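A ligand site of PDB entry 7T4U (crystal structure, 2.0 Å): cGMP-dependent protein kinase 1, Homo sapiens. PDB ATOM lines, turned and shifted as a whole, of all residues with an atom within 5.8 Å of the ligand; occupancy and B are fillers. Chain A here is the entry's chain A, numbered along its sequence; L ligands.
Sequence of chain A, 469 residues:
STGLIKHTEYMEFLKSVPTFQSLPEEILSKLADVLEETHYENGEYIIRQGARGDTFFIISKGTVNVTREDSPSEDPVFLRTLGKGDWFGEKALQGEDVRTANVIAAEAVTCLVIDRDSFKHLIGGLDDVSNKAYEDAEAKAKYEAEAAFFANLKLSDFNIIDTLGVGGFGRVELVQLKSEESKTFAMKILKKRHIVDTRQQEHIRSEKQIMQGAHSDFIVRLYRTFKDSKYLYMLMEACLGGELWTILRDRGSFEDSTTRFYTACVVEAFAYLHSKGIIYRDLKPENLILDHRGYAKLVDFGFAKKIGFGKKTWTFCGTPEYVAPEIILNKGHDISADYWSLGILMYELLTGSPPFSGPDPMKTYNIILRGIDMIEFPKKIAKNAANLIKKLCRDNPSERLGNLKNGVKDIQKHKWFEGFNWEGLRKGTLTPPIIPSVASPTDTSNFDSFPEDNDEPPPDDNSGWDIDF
The backbone carbonyl oxygen (O) of Ala 141 is in hydrogen-bond range of a nitrogen (N1) of the ligand.
The side-chain amide nitrogen (NE2) of Gln 94 sits at hydrogen-bond distance from an oxygen (O3) of the ligand (3.3 Å).
The backbone carbonyl oxygen (O) of Ile 114 lies within hydrogen-bond range of the backbone NH (N) of Phe 56 (3.2 Å).
Merely in contact with the ligand: Thr 19 (3.8 Å), Phe 20 (3.5 Å), Leu 23 (3.4 Å), Leu 31 (3.8 Å), Phe 56 (3.5 Å), Trp 87 (3.7 Å), Glu 90 (3.7 Å), Leu 93 (3.6 Å), Ile 114 (3.9 Å), Phe 119 (3.6 Å), Tyr 134 (3.6 Å) and Ala 137 (3.5 Å).
Hydrophobic or aromatic side chains within 4 Å of the ligand: Phe 20, Leu 23, Leu 31, Phe 56, Trp 87, Leu 93, Ile 114, Phe 119, Tyr 134, Ala 137 and Ala 141.
14 residues have an atom within 4 Å of the ligand: Thr 19, Phe 20, Leu 23, Leu 31, Phe 56, Trp 87, Glu 90, Leu 93, Gln 94, Ile 114, Phe 119, Tyr 134, Ala 137 and Ala 141.
Along chain A the residues within 4 Å of the ligand span positions 19 to 141.
The nearest printed residue that does not touch the ligand is Ala 145 (4.03 Å).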
ATOM      1  N   THR A  19      12.734 -12.933  29.799  1.00  0.00           N
ATOM      2  CA  THR A  19      11.773 -12.050  29.135  1.00  0.00           C
ATOM      3  C   THR A  19      11.557 -10.711  29.876  1.00  0.00           C
ATOM      4  O   THR A  19      11.574  -9.650  29.245  1.00  0.00           O
ATOM      5  CB  THR A  19      10.421 -12.750  28.966  1.00  0.00           C
ATOM      6  OG1 THR A  19      10.631 -14.140  28.665  1.00  0.00           O
ATOM      7  CG2 THR A  19       9.561 -12.114  27.893  1.00  0.00           C
ATOM      8  N   PHE A  20      11.323 -10.774  31.196  1.00  0.00           N
ATOM      9  CA  PHE A  20      10.999  -9.584  31.998  1.00  0.00           C
ATOM     10  C   PHE A  20      12.175  -8.645  32.300  1.00  0.00           C
ATOM     11  O   PHE A  20      11.931  -7.456  32.467  1.00  0.00           O
ATOM     12  CB  PHE A  20      10.314  -9.986  33.325  1.00  0.00           C
ATOM     13  CG  PHE A  20       9.044 -10.803  33.182  1.00  0.00           C
ATOM     14  CD1 PHE A  20       7.991 -10.329  32.417  1.00  0.00           C
ATOM     15  CD2 PHE A  20       8.889 -12.006  33.844  1.00  0.00           C
ATOM     16  CE1 PHE A  20       6.832 -11.095  32.259  1.00  0.00           C
ATOM     17  CE2 PHE A  20       7.718 -12.754  33.709  1.00  0.00           C
ATOM     18  CZ  PHE A  20       6.696 -12.295  32.907  1.00  0.00           C
ATOM     19  N   LEU A  23      12.485  -5.133  30.577  1.00  0.00           N
ATOM     20  CA  LEU A  23      11.473  -4.131  30.901  1.00  0.00           C
ATOM     21  C   LEU A  23      11.977  -3.004  31.827  1.00  0.00           C
ATOM     22  O   LEU A  23      12.893  -3.214  32.619  1.00  0.00           O
ATOM     23  CB  LEU A  23      10.209  -4.789  31.495  1.00  0.00           C
ATOM     24  CG  LEU A  23       9.498  -5.852  30.615  1.00  0.00           C
ATOM     25  CD1 LEU A  23       8.344  -6.487  31.358  1.00  0.00           C
ATOM     26  CD2 LEU A  23       9.014  -5.249  29.323  1.00  0.00           C
ATOM     27  N   ILE A  27       7.702  -0.652  35.327  1.00  0.00           N
ATOM     28  CA  ILE A  27       6.837  -1.825  35.096  1.00  0.00           C
ATOM     29  C   ILE A  27       7.182  -2.929  36.107  1.00  0.00           C
ATOM     30  O   ILE A  27       6.286  -3.448  36.770  1.00  0.00           O
ATOM     31  CB  ILE A  27       6.969  -2.352  33.627  1.00  0.00           C
ATOM     32  CG1 ILE A  27       6.746  -1.206  32.584  1.00  0.00           C
ATOM     33  CG2 ILE A  27       6.009  -3.533  33.367  1.00  0.00           C
ATOM     34  CD1 ILE A  27       6.556  -1.664  31.130  1.00  0.00           C
ATOM     35  N   LEU A  31       4.778  -4.213  38.981  1.00  0.00           N
ATOM     36  CA  LEU A  31       4.444  -5.655  38.997  1.00  0.00           C
ATOM     37  C   LEU A  31       4.676  -6.189  40.411  1.00  0.00           C
ATOM     38  O   LEU A  31       3.750  -6.742  41.014  1.00  0.00           O
ATOM     39  CB  LEU A  31       5.278  -6.458  37.987  1.00  0.00           C
ATOM     40  CG  LEU A  31       4.826  -6.388  36.530  1.00  0.00           C
ATOM     41  CD1 LEU A  31       5.917  -6.904  35.598  1.00  0.00           C
ATOM     42  CD2 LEU A  31       3.519  -7.168  36.324  1.00  0.00           C
ATOM     43  N   LEU A  35       2.000  -8.386  42.479  1.00  0.00           N
ATOM     44  CA  LEU A  35       2.115  -9.852  42.372  1.00  0.00           C
ATOM     45  C   LEU A  35       1.897 -10.509  43.755  1.00  0.00           C
ATOM     46  O   LEU A  35       2.365  -9.968  44.752  1.00  0.00           O
ATOM     47  CB  LEU A  35       3.504 -10.284  41.819  1.00  0.00           C
ATOM     48  CG  LEU A  35       3.705 -10.107  40.324  1.00  0.00           C
ATOM     49  CD1 LEU A  35       5.173 -10.024  39.993  1.00  0.00           C
ATOM     50  CD2 LEU A  35       3.053 -11.242  39.536  1.00  0.00           C
ATOM     51  N   PHE A  56      -2.507 -15.510  35.560  1.00  0.00           N
ATOM     52  CA  PHE A  56      -1.205 -15.804  34.943  1.00  0.00           C
ATOM     53  C   PHE A  56      -0.235 -16.175  36.070  1.00  0.00           C
ATOM     54  O   PHE A  56      -0.230 -15.510  37.094  1.00  0.00           O
ATOM     55  CB  PHE A  56      -0.691 -14.572  34.199  1.00  0.00           C
ATOM     56  CG  PHE A  56       0.730 -14.662  33.688  1.00  0.00           C
ATOM     57  CD1 PHE A  56       1.045 -15.465  32.602  1.00  0.00           C
ATOM     58  CD2 PHE A  56       1.723 -13.854  34.222  1.00  0.00           C
ATOM     59  CE1 PHE A  56       2.343 -15.514  32.093  1.00  0.00           C
ATOM     60  CE2 PHE A  56       3.033 -13.913  33.726  1.00  0.00           C
ATOM     61  CZ  PHE A  56       3.329 -14.735  32.657  1.00  0.00           C
ATOM     62  N   ILE A  58       3.851 -17.175  37.342  1.00  0.00           N
ATOM     63  CA  ILE A  58       5.292 -17.192  37.098  1.00  0.00           C
ATOM     64  C   ILE A  58       5.819 -18.096  38.205  1.00  0.00           C
ATOM     65  O   ILE A  58       5.512 -17.853  39.357  1.00  0.00           O
ATOM     66  CB  ILE A  58       5.991 -15.802  37.163  1.00  0.00           C
ATOM     67  CG1 ILE A  58       5.369 -14.792  36.158  1.00  0.00           C
ATOM     68  CG2 ILE A  58       7.502 -15.967  36.900  1.00  0.00           C
ATOM     69  CD1 ILE A  58       5.644 -13.357  36.523  1.00  0.00           C
ATOM     70  N   TRP A  87       6.695 -19.606  33.062  1.00  0.00           N
ATOM     71  CA  TRP A  87       5.359 -19.121  33.318  1.00  0.00           C
ATOM     72  C   TRP A  87       4.318 -19.797  32.452  1.00  0.00           C
ATOM     73  O   TRP A  87       4.658 -20.444  31.473  1.00  0.00           O
ATOM     74  CB  TRP A  87       5.308 -17.594  33.108  1.00  0.00           C
ATOM     75  CG  TRP A  87       6.182 -17.082  32.002  1.00  0.00           C
ATOM     76  CD1 TRP A  87       7.420 -16.507  32.131  1.00  0.00           C
ATOM     77  CD2 TRP A  87       5.870 -17.060  30.599  1.00  0.00           C
ATOM     78  NE1 TRP A  87       7.888 -16.115  30.896  1.00  0.00           N
ATOM     79  CE2 TRP A  87       6.952 -16.428  29.947  1.00  0.00           C
ATOM     80  CE3 TRP A  87       4.789 -17.513  29.842  1.00  0.00           C
ATOM     81  CZ2 TRP A  87       6.971 -16.247  28.555  1.00  0.00           C
ATOM     82  CZ3 TRP A  87       4.818 -17.359  28.466  1.00  0.00           C
ATOM     83  CH2 TRP A  87       5.902 -16.735  27.837  1.00  0.00           C
ATOM     84  N   GLU A  90      -1.241 -17.397  30.556  1.00  0.00           N
ATOM     85  CA  GLU A  90      -1.315 -16.028  30.006  1.00  0.00           C
ATOM     86  C   GLU A  90      -2.581 -15.667  29.223  1.00  0.00           C
ATOM     87  O   GLU A  90      -2.896 -14.484  29.128  1.00  0.00           O
ATOM     88  CB  GLU A  90      -0.076 -15.736  29.116  1.00  0.00           C
ATOM     89  CG  GLU A  90       0.091 -16.667  27.911  1.00  0.00           C
ATOM     90  CD  GLU A  90       1.246 -17.654  27.945  1.00  0.00           C
ATOM     91  OE1 GLU A  90       1.578 -18.164  29.044  1.00  0.00           O
ATOM     92  OE2 GLU A  90       1.805 -17.936  26.862  1.00  0.00           O
ATOM     93  N   LYS A  91      -3.261 -16.649  28.620  1.00  0.00           N
ATOM     94  CA  LYS A  91      -4.458 -16.370  27.822  1.00  0.00           C
ATOM     95  C   LYS A  91      -5.616 -15.861  28.702  1.00  0.00           C
ATOM     96  O   LYS A  91      -6.438 -15.078  28.222  1.00  0.00           O
ATOM     97  CB  LYS A  91      -4.858 -17.608  26.980  1.00  0.00           C
ATOM     98  CG  LYS A  91      -4.206 -17.631  25.580  1.00  0.00           C
ATOM     99  CD  LYS A  91      -2.659 -17.612  25.635  1.00  0.00           C
ATOM    100  CE  LYS A  91      -1.995 -17.786  24.281  1.00  0.00           C
ATOM    101  NZ  LYS A  91      -1.977 -19.207  23.835  1.00  0.00           N
ATOM    102  N   LEU A  93      -5.368 -13.611  30.962  1.00  0.00           N
ATOM    103  CA  LEU A  93      -5.174 -12.155  31.048  1.00  0.00           C
ATOM    104  C   LEU A  93      -5.798 -11.474  29.831  1.00  0.00           C
ATOM    105  O   LEU A  93      -6.359 -10.385  29.960  1.00  0.00           O
ATOM    106  CB  LEU A  93      -3.681 -11.781  31.049  1.00  0.00           C
ATOM    107  CG  LEU A  93      -2.801 -12.363  32.130  1.00  0.00           C
ATOM    108  CD1 LEU A  93      -1.400 -11.835  31.989  1.00  0.00           C
ATOM    109  CD2 LEU A  93      -3.348 -12.078  33.510  1.00  0.00           C
ATOM    110  N   GLN A  94      -5.640 -12.096  28.635  1.00  0.00           N
ATOM    111  CA  GLN A  94      -6.183 -11.555  27.380  1.00  0.00           C
ATOM    112  C   GLN A  94      -7.707 -11.740  27.227  1.00  0.00           C
ATOM    113  O   GLN A  94      -8.256 -11.173  26.285  1.00  0.00           O
ATOM    114  CB  GLN A  94      -5.443 -12.121  26.139  1.00  0.00           C
ATOM    115  CG  GLN A  94      -4.477 -11.114  25.517  1.00  0.00           C
ATOM    116  CD  GLN A  94      -3.282 -10.833  26.382  1.00  0.00           C
ATOM    117  OE1 GLN A  94      -3.347 -10.068  27.358  1.00  0.00           O
ATOM    118  NE2 GLN A  94      -2.150 -11.457  26.065  1.00  0.00           N
ATOM    119  N   ILE A 114      -0.883 -12.959  39.106  1.00  0.00           N
ATOM    120  CA  ILE A 114      -1.537 -11.689  38.810  1.00  0.00           C
ATOM    121  C   ILE A 114      -2.787 -12.028  37.996  1.00  0.00           C
ATOM    122  O   ILE A 114      -2.680 -12.584  36.894  1.00  0.00           O
ATOM    123  CB  ILE A 114      -0.639 -10.614  38.130  1.00  0.00           C
ATOM    124  CG1 ILE A 114      -1.360  -9.232  38.129  1.00  0.00           C
ATOM    125  CG2 ILE A 114      -0.209 -11.011  36.725  1.00  0.00           C
ATOM    126  CD1 ILE A 114      -0.533  -8.095  37.604  1.00  0.00           C
ATOM    127  N   PHE A 119      -3.933  -7.191  36.312  1.00  0.00           N
ATOM    128  CA  PHE A 119      -3.053  -6.972  35.150  1.00  0.00           C
ATOM    129  C   PHE A 119      -3.650  -5.865  34.285  1.00  0.00           C
ATOM    130  O   PHE A 119      -2.919  -4.986  33.837  1.00  0.00           O
ATOM    131  CB  PHE A 119      -2.862  -8.266  34.296  1.00  0.00           C
ATOM    132  CG  PHE A 119      -2.051  -8.053  33.022  1.00  0.00           C
ATOM    133  CD1 PHE A 119      -0.656  -7.953  33.073  1.00  0.00           C
ATOM    134  CD2 PHE A 119      -2.671  -7.857  31.792  1.00  0.00           C
ATOM    135  CE1 PHE A 119       0.084  -7.662  31.920  1.00  0.00           C
ATOM    136  CE2 PHE A 119      -1.918  -7.565  30.643  1.00  0.00           C
ATOM    137  CZ  PHE A 119      -0.548  -7.473  30.710  1.00  0.00           C
ATOM    138  N   TYR A 134       7.934  -2.099  25.900  1.00  0.00           N
ATOM    139  CA  TYR A 134       6.904  -3.130  26.012  1.00  0.00           C
ATOM    140  C   TYR A 134       6.628  -3.673  24.586  1.00  0.00           C
ATOM    141  O   TYR A 134       6.603  -4.891  24.389  1.00  0.00           O
ATOM    142  CB  TYR A 134       5.626  -2.515  26.618  1.00  0.00           C
ATOM    143  CG  TYR A 134       4.500  -3.482  26.891  1.00  0.00           C
ATOM    144  CD1 TYR A 134       4.456  -4.229  28.054  1.00  0.00           C
ATOM    145  CD2 TYR A 134       3.383  -3.518  26.064  1.00  0.00           C
ATOM    146  CE1 TYR A 134       3.382  -5.058  28.355  1.00  0.00           C
ATOM    147  CE2 TYR A 134       2.290  -4.342  26.355  1.00  0.00           C
ATOM    148  CZ  TYR A 134       2.291  -5.110  27.507  1.00  0.00           C
ATOM    149  OH  TYR A 134       1.228  -5.924  27.824  1.00  0.00           O
ATOM    150  N   ALA A 137       9.486  -5.998  23.300  1.00  0.00           N
ATOM    151  CA  ALA A 137       9.368  -7.303  23.931  1.00  0.00           C
ATOM    152  C   ALA A 137       8.142  -8.054  23.401  1.00  0.00           C
ATOM    153  O   ALA A 137       8.210  -9.275  23.242  1.00  0.00           O
ATOM    154  CB  ALA A 137       9.264  -7.140  25.440  1.00  0.00           C
ATOM    155  N   GLU A 138       7.024  -7.329  23.108  1.00  0.00           N
ATOM    156  CA  GLU A 138       5.810  -7.949  22.558  1.00  0.00           C
ATOM    157  C   GLU A 138       6.095  -8.441  21.117  1.00  0.00           C
ATOM    158  O   GLU A 138       5.704  -9.549  20.776  1.00  0.00           O
ATOM    159  CB  GLU A 138       4.603  -6.994  22.591  1.00  0.00           C
ATOM    160  CG  GLU A 138       3.276  -7.739  22.536  1.00  0.00           C
ATOM    161  CD  GLU A 138       2.046  -6.853  22.416  1.00  0.00           C
ATOM    162  OE1 GLU A 138       1.059  -7.107  23.158  1.00  0.00           O
ATOM    163  OE2 GLU A 138       2.057  -5.916  21.591  1.00  0.00           O
ATOM    164  N   ALA A 141       8.387 -11.627  21.248  1.00  0.00           N
ATOM    165  CA  ALA A 141       7.622 -12.823  21.629  1.00  0.00           C
ATOM    166  C   ALA A 141       6.493 -13.178  20.636  1.00  0.00           C
ATOM    167  O   ALA A 141       6.052 -14.330  20.612  1.00  0.00           O
ATOM    168  CB  ALA A 141       7.063 -12.645  23.001  1.00  0.00           C
ATOM    169  N   LYS A 142       6.006 -12.188  19.862  1.00  0.00           N
ATOM    170  CA  LYS A 142       4.990 -12.400  18.816  1.00  0.00           C
ATOM    171  C   LYS A 142       5.668 -13.170  17.631  1.00  0.00           C
ATOM    172  O   LYS A 142       5.007 -14.033  17.039  1.00  0.00           O
ATOM    173  CB  LYS A 142       4.405 -11.036  18.376  1.00  0.00           C
ATOM    174  CG  LYS A 142       3.415 -11.048  17.210  1.00  0.00           C
ATOM    175  CD  LYS A 142       3.720  -9.898  16.239  1.00  0.00           C
ATOM    176  CE  LYS A 142       2.809  -9.853  15.045  1.00  0.00           C
ATOM    177  NZ  LYS A 142       3.064  -8.661  14.196  1.00  0.00           N
ATOM    178  N   ALA A 145       6.575 -16.870  18.722  1.00  0.00           N
ATOM    179  CA  ALA A 145       5.321 -17.629  18.729  1.00  0.00           C
ATOM    180  C   ALA A 145       4.920 -17.983  17.279  1.00  0.00           C
ATOM    181  O   ALA A 145       4.381 -19.059  17.047  1.00  0.00           O
ATOM    182  CB  ALA A 145       4.229 -16.838  19.410  1.00  0.00           C
HETATM  183  C1  LIG L   1       5.808  -7.727  26.997  1.00  0.00           C
HETATM  184  C2  LIG L   1       4.507  -8.114  26.756  1.00  0.00           C
HETATM  185  C3  LIG L   1       6.765  -8.673  27.327  1.00  0.00           C
HETATM  186  C4  LIG L   1       1.962 -11.970  22.276  1.00  0.00           C
HETATM  187  C5  LIG L   1       4.150  -9.447  26.843  1.00  0.00           C
HETATM  188  C6  LIG L   1       6.397  -9.997  27.431  1.00  0.00           C
HETATM  189  C7  LIG L   1       2.825 -11.752  23.325  1.00  0.00           C
HETATM  190  C8  LIG L   1       2.751 -14.209  22.084  1.00  0.00           C
HETATM  191  C9  LIG L   1       2.650 -10.816  32.184  1.00  0.00           C
HETATM  192  C10 LIG L   1       3.463  -9.298  30.535  1.00  0.00           C
HETATM  193  C11 LIG L   1       4.032  -9.005  32.845  1.00  0.00           C
HETATM  194  C12 LIG L   1       1.920 -13.201  21.642  1.00  0.00           C
HETATM  195  C13 LIG L   1       5.096 -10.401  27.194  1.00  0.00           C
HETATM  196  C14 LIG L   1       3.669 -12.760  23.770  1.00  0.00           C
HETATM  197  C15 LIG L   1       2.732 -10.424  30.862  1.00  0.00           C
HETATM  198  C16 LIG L   1       3.635 -14.003  23.136  1.00  0.00           C
HETATM  199  C17 LIG L   1       3.302 -10.113  33.169  1.00  0.00           C
HETATM  200  C18 LIG L   1       4.105  -8.594  31.530  1.00  0.00           C
HETATM  201  C19 LIG L   1       0.955 -13.438  20.531  1.00  0.00           C
HETATM  202  C20 LIG L   1       3.101 -14.159  28.007  1.00  0.00           C
HETATM  203  C21 LIG L   1       3.954 -13.493  29.062  1.00  0.00           C
HETATM  204  C22 LIG L   1       3.644 -13.942  26.607  1.00  0.00           C
HETATM  205  C23 LIG L   1       4.751 -11.844  27.357  1.00  0.00           C
HETATM  206  C24 LIG L   1       4.101 -12.035  28.719  1.00  0.00           C
HETATM  207  C25 LIG L   1       4.555 -12.415  24.939  1.00  0.00           C
HETATM  208  C26 LIG L   1       0.759 -10.546  29.366  1.00  0.00           C
HETATM  209  C27 LIG L   1       2.030 -11.230  29.813  1.00  0.00           C
HETATM  210  N1  LIG L   1       4.430 -15.099  23.514  1.00  0.00           N
HETATM  211  N2  LIG L   1       3.909 -12.503  26.282  1.00  0.00           N
HETATM  212  O1  LIG L   1       0.622 -14.646  20.355  1.00  0.00           O
HETATM  213  O2  LIG L   1       0.529 -12.446  19.873  1.00  0.00           O
HETATM  214  O3  LIG L   1       0.037 -11.493  28.597  1.00  0.00           O
HETATM  215  O4  LIG L   1       2.823 -11.377  28.624  1.00  0.00           O
HETATM  216 CL1  LIG L   1       3.209 -10.599  34.828  1.00  0.00          CL
HETATM  217 CL2  LIG L   1       5.034  -7.214  31.095  1.00  0.00          CL
